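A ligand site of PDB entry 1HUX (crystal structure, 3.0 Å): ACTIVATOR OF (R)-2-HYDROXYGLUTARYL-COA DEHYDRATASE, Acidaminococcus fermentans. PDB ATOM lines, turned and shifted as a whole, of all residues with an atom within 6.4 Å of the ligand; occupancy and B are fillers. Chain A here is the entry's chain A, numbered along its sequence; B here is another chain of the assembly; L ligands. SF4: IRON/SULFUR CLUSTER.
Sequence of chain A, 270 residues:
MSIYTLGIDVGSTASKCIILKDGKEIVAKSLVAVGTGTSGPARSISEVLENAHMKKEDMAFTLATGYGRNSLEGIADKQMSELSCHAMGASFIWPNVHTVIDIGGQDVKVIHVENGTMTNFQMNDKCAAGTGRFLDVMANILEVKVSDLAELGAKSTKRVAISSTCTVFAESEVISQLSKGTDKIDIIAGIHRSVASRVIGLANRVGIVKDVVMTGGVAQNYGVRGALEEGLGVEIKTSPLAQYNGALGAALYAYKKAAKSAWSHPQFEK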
ATOM      1  N   LYS A 126      24.579  -9.968  18.860  1.00  0.00           N
ATOM      2  CA  LYS A 126      23.710  -9.398  17.840  1.00  0.00           C
ATOM      3  C   LYS A 126      22.869  -8.185  18.243  1.00  0.00           C
ATOM      4  O   LYS A 126      22.660  -7.273  17.447  1.00  0.00           O
ATOM      5  CB  LYS A 126      22.771 -10.480  17.319  1.00  0.00           C
ATOM      6  CG  LYS A 126      23.468 -11.769  16.924  1.00  0.00           C
ATOM      7  CD  LYS A 126      22.445 -12.832  16.569  1.00  0.00           C
ATOM      8  CE  LYS A 126      23.109 -14.161  16.254  1.00  0.00           C
ATOM      9  NZ  LYS A 126      22.109 -15.213  15.943  1.00  0.00           N
ATOM     10  N   CYS A 127      22.392  -8.163  19.477  1.00  0.00           N
ATOM     11  CA  CYS A 127      21.558  -7.066  19.943  1.00  0.00           C
ATOM     12  C   CYS A 127      22.422  -5.969  20.581  1.00  0.00           C
ATOM     13  O   CYS A 127      23.274  -6.254  21.419  1.00  0.00           O
ATOM     14  CB  CYS A 127      20.515  -7.602  20.950  1.00  0.00           C
ATOM     15  SG  CYS A 127      19.282  -6.396  21.521  1.00  0.00           S
ATOM     16  N   ALA A 128      22.206  -4.728  20.175  1.00  0.00           N
ATOM     17  CA  ALA A 128      22.937  -3.591  20.722  1.00  0.00           C
ATOM     18  C   ALA A 128      22.488  -3.306  22.153  1.00  0.00           C
ATOM     19  O   ALA A 128      23.139  -2.543  22.870  1.00  0.00           O
ATOM     20  CB  ALA A 128      22.706  -2.358  19.863  1.00  0.00           C
ATOM     21  N   ALA A 129      21.377  -3.903  22.568  1.00  0.00           N
ATOM     22  CA  ALA A 129      20.869  -3.696  23.923  1.00  0.00           C
ATOM     23  C   ALA A 129      21.837  -4.237  24.959  1.00  0.00           C
ATOM     24  O   ALA A 129      22.465  -5.277  24.755  1.00  0.00           O
ATOM     25  CB  ALA A 129      19.489  -4.360  24.076  1.00  0.00           C
ATOM     26  N   THR A 165      12.907  -2.642  25.519  1.00  0.00           N
ATOM     27  CA  THR A 165      14.062  -3.541  25.611  1.00  0.00           C
ATOM     28  C   THR A 165      15.078  -3.205  24.524  1.00  0.00           C
ATOM     29  O   THR A 165      16.271  -3.488  24.642  1.00  0.00           O
ATOM     30  CB  THR A 165      13.645  -4.975  25.336  1.00  0.00           C
ATOM     31  OG1 THR A 165      12.309  -5.196  25.756  1.00  0.00           O
ATOM     32  CG2 THR A 165      14.496  -5.908  26.118  1.00  0.00           C
ATOM     33  N   CYS A 166      14.572  -2.624  23.443  1.00  0.00           N
ATOM     34  CA  CYS A 166      15.412  -2.265  22.309  1.00  0.00           C
ATOM     35  C   CYS A 166      16.055  -0.888  22.439  1.00  0.00           C
ATOM     36  O   CYS A 166      15.451   0.025  22.987  1.00  0.00           O
ATOM     37  CB  CYS A 166      14.580  -2.287  21.041  1.00  0.00           C
ATOM     38  SG  CYS A 166      15.466  -1.631  19.645  1.00  0.00           S
ATOM     39  N   THR A 167      17.268  -0.753  21.920  1.00  0.00           N
ATOM     40  CA  THR A 167      17.957   0.538  21.955  1.00  0.00           C
ATOM     41  C   THR A 167      17.184   1.560  21.140  1.00  0.00           C
ATOM     42  O   THR A 167      17.040   2.719  21.552  1.00  0.00           O
ATOM     43  CB  THR A 167      19.352   0.460  21.307  1.00  0.00           C
ATOM     44  OG1 THR A 167      19.564  -0.823  20.734  1.00  0.00           O
ATOM     45  CG2 THR A 167      20.393   0.583  22.320  1.00  0.00           C
ATOM     46  N   VAL A 168      16.723   1.156  19.969  1.00  0.00           N
ATOM     47  CA  VAL A 168      15.977   2.060  19.087  1.00  0.00           C
ATOM     48  C   VAL A 168      14.679   2.565  19.707  1.00  0.00           C
ATOM     49  O   VAL A 168      14.403   3.766  19.742  1.00  0.00           O
ATOM     50  CB  VAL A 168      15.647   1.401  17.739  1.00  0.00           C
ATOM     51  CG1 VAL A 168      14.924   2.402  16.844  1.00  0.00           C
ATOM     52  CG2 VAL A 168      16.926   0.899  17.074  1.00  0.00           C
ATOM     53  N   PHE A 169      13.859   1.637  20.188  1.00  0.00           N
ATOM     54  CA  PHE A 169      12.620   2.034  20.809  1.00  0.00           C
ATOM     55  C   PHE A 169      12.907   2.787  22.100  1.00  0.00           C
ATOM     56  O   PHE A 169      12.302   3.818  22.361  1.00  0.00           O
ATOM     57  CB  PHE A 169      11.755   0.787  21.043  1.00  0.00           C
ATOM     58  CG  PHE A 169      11.253   0.155  19.771  1.00  0.00           C
ATOM     59  CD1 PHE A 169      10.995  -1.197  19.694  1.00  0.00           C
ATOM     60  CD2 PHE A 169      11.077   0.928  18.615  1.00  0.00           C
ATOM     61  CE1 PHE A 169      10.558  -1.797  18.494  1.00  0.00           C
ATOM     62  CE2 PHE A 169      10.646   0.356  17.413  1.00  0.00           C
ATOM     63  CZ  PHE A 169      10.387  -1.017  17.359  1.00  0.00           C
ATOM     64  N   LYS B 126       9.207  -6.058  20.153  1.00  0.00           N
ATOM     65  CA  LYS B 126      10.368  -5.539  20.869  1.00  0.00           C
ATOM     66  C   LYS B 126      11.566  -5.058  20.041  1.00  0.00           C
ATOM     67  O   LYS B 126      12.208  -4.077  20.400  1.00  0.00           O
ATOM     68  CB  LYS B 126      10.858  -6.591  21.866  1.00  0.00           C
ATOM     69  CG  LYS B 126       9.773  -7.197  22.727  1.00  0.00           C
ATOM     70  CD  LYS B 126      10.326  -8.344  23.550  1.00  0.00           C
ATOM     71  CE  LYS B 126       9.230  -9.014  24.364  1.00  0.00           C
ATOM     72  NZ  LYS B 126       9.760 -10.172  25.142  1.00  0.00           N
ATOM     73  N   CYS B 127      11.861  -5.751  18.953  1.00  0.00           N
ATOM     74  CA  CYS B 127      13.000  -5.396  18.104  1.00  0.00           C
ATOM     75  C   CYS B 127      12.567  -4.411  17.011  1.00  0.00           C
ATOM     76  O   CYS B 127      11.565  -4.645  16.322  1.00  0.00           O
ATOM     77  CB  CYS B 127      13.585  -6.685  17.472  1.00  0.00           C
ATOM     78  SG  CYS B 127      15.176  -6.551  16.507  1.00  0.00           S
ATOM     79  N   ALA B 128      13.306  -3.305  16.877  1.00  0.00           N
ATOM     80  CA  ALA B 128      13.016  -2.298  15.863  1.00  0.00           C
ATOM     81  C   ALA B 128      13.339  -2.822  14.468  1.00  0.00           C
ATOM     82  O   ALA B 128      12.947  -2.233  13.480  1.00  0.00           O
ATOM     83  CB  ALA B 128      13.833  -1.033  16.139  1.00  0.00           C
ATOM     84  N   ALA B 129      14.053  -3.933  14.410  1.00  0.00           N
ATOM     85  CA  ALA B 129      14.416  -4.519  13.110  1.00  0.00           C
ATOM     86  C   ALA B 129      13.188  -4.981  12.355  1.00  0.00           C
ATOM     87  O   ALA B 129      12.235  -5.475  12.956  1.00  0.00           O
ATOM     88  CB  ALA B 129      15.370  -5.688  13.319  1.00  0.00           C
ATOM     89  N   THR B 165      21.834  -7.599  11.654  1.00  0.00           N
ATOM     90  CA  THR B 165      20.430  -7.878  11.892  1.00  0.00           C
ATOM     91  C   THR B 165      19.792  -6.739  12.649  1.00  0.00           C
ATOM     92  O   THR B 165      18.575  -6.542  12.595  1.00  0.00           O
ATOM     93  CB  THR B 165      20.289  -9.099  12.768  1.00  0.00           C
ATOM     94  OG1 THR B 165      21.354 -10.008  12.516  1.00  0.00           O
ATOM     95  CG2 THR B 165      19.008  -9.829  12.435  1.00  0.00           C
ATOM     96  N   CYS B 166      20.619  -6.056  13.428  1.00  0.00           N
ATOM     97  CA  CYS B 166      20.177  -4.957  14.268  1.00  0.00           C
ATOM     98  C   CYS B 166      20.100  -3.600  13.541  1.00  0.00           C
ATOM     99  O   CYS B 166      20.934  -3.315  12.699  1.00  0.00           O
ATOM    100  CB  CYS B 166      21.140  -4.823  15.450  1.00  0.00           C
ATOM    101  SG  CYS B 166      20.834  -3.384  16.471  1.00  0.00           S
ATOM    102  N   THR B 167      19.094  -2.781  13.875  1.00  0.00           N
ATOM    103  CA  THR B 167      18.969  -1.468  13.255  1.00  0.00           C
ATOM    104  C   THR B 167      20.175  -0.612  13.613  1.00  0.00           C
ATOM    105  O   THR B 167      20.685   0.131  12.780  1.00  0.00           O
ATOM    106  CB  THR B 167      17.759  -0.654  13.773  1.00  0.00           C
ATOM    107  OG1 THR B 167      17.135  -1.330  14.864  1.00  0.00           O
ATOM    108  CG2 THR B 167      16.720  -0.560  12.761  1.00  0.00           C
ATOM    109  N   VAL B 168      20.612  -0.684  14.872  1.00  0.00           N
ATOM    110  CA  VAL B 168      21.749   0.126  15.334  1.00  0.00           C
ATOM    111  C   VAL B 168      23.046  -0.251  14.641  1.00  0.00           C
ATOM    112  O   VAL B 168      23.770   0.610  14.126  1.00  0.00           O
ATOM    113  CB  VAL B 168      21.969   0.018  16.840  1.00  0.00           C
ATOM    114  CG1 VAL B 168      23.140   0.899  17.250  1.00  0.00           C
ATOM    115  CG2 VAL B 168      20.696   0.421  17.586  1.00  0.00           C
ATOM    116  N   PHE B 169      23.358  -1.532  14.630  1.00  0.00           N
ATOM    117  CA  PHE B 169      24.569  -1.968  13.967  1.00  0.00           C
ATOM    118  C   PHE B 169      24.438  -1.757  12.459  1.00  0.00           C
ATOM    119  O   PHE B 169      25.364  -1.251  11.821  1.00  0.00           O
ATOM    120  CB  PHE B 169      24.854  -3.431  14.314  1.00  0.00           C
ATOM    121  CG  PHE B 169      25.233  -3.641  15.768  1.00  0.00           C
ATOM    122  CD1 PHE B 169      24.959  -4.850  16.423  1.00  0.00           C
ATOM    123  CD2 PHE B 169      25.827  -2.611  16.502  1.00  0.00           C
ATOM    124  CE1 PHE B 169      25.275  -5.021  17.799  1.00  0.00           C
ATOM    125  CE2 PHE B 169      26.144  -2.783  17.869  1.00  0.00           C
ATOM    126  CZ  PHE B 169      25.867  -3.984  18.512  1.00  0.00           C
HETATM  127 FE1  SF4 L   1      16.879  -3.257  18.992  1.00  0.00          FE
HETATM  128 FE2  SF4 L   1      16.763  -5.420  17.664  1.00  0.00          FE
HETATM  129 FE3  SF4 L   1      19.005  -4.006  17.647  1.00  0.00          FE
HETATM  130 FE4  SF4 L   1      18.372  -5.290  19.751  1.00  0.00          FE
HETATM  131  S1  SF4 L   1      18.888  -6.295  17.772  1.00  0.00           S
HETATM  132  S2  SF4 L   1      19.042  -3.113  19.725  1.00  0.00           S
HETATM  133  S3  SF4 L   1      16.079  -5.198  19.780  1.00  0.00           S
HETATM  134  S4  SF4 L   1      17.012  -3.362  16.736  1.00  0.00           S
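The side-chain sulfur (SG) of Cys 166 of chain B sits close to the backbone NH (N) of Val 168 of chain B (3.1 Å). N of Ala 129 of chain A sits close to SG of Cys 127 of chain A (3.4 Å). SG of Cys 166 of chain A sits close to N of Phe 169 of chain A. N of Ala 129 of chain B sits close to SG of Cys 127 of chain B (3.5 Å). SG of Cys 166 of chain A lies close to N of Val 168 of chain A, 3.1 Å away. The side-chain sulfur (SG) of Cys 166 of chain B sits close to the backbone NH (N) of Phe 169 of chain B, at 3.6 Å.
O of Lys 126 of chain A touches S1 of the ligand (3.9 Å). Ala 129 of chain B touches the ligand (N to S4, 3.8 Å). Hydrophobic or aromatic side chains within 4 Å of the ligand: Ala 128 of chain A and Ala 128 of chain B. Along chain A the residues within 4 Å of the ligand span positions 126 to 167.
SG of Cys 127 of chain A binds FE4 of the ligand, 2.3 Å away. N of Ala 128 of chain A sits close to S2 of the ligand (3.6 Å). The side-chain sulfur (SG) of Cys 127 of chain B is bound to an iron atom (FE2) of the ligand, 2.3 Å away. The side-chain sulfur of Cys 166 of chain A is bound to an iron atom (FE1) of the ligand, at 2.3 Å. S4 of the ligand sits close to N of Ala 128 of chain B (3.7 Å). OG1 of Thr 167 of chain A sits close to S2 of the ligand (2.6 Å). S2 of the ligand sits close to N of Thr 167 of chain A, 3.7 Å away. OG1 of Thr 167 of chain B lies close to S4 of the ligand. The backbone NH (N) of Ala 129 of chain A sits close to a sulfur (S2) of the ligand, 3.8 Å away. The backbone NH of Thr 167 of chain B lies close to a sulfur (S4) of the ligand (3.6 Å). The side-chain sulfur of Cys 166 of chain B is bound to an iron atom (FE3) of the ligand (2.3 Å).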
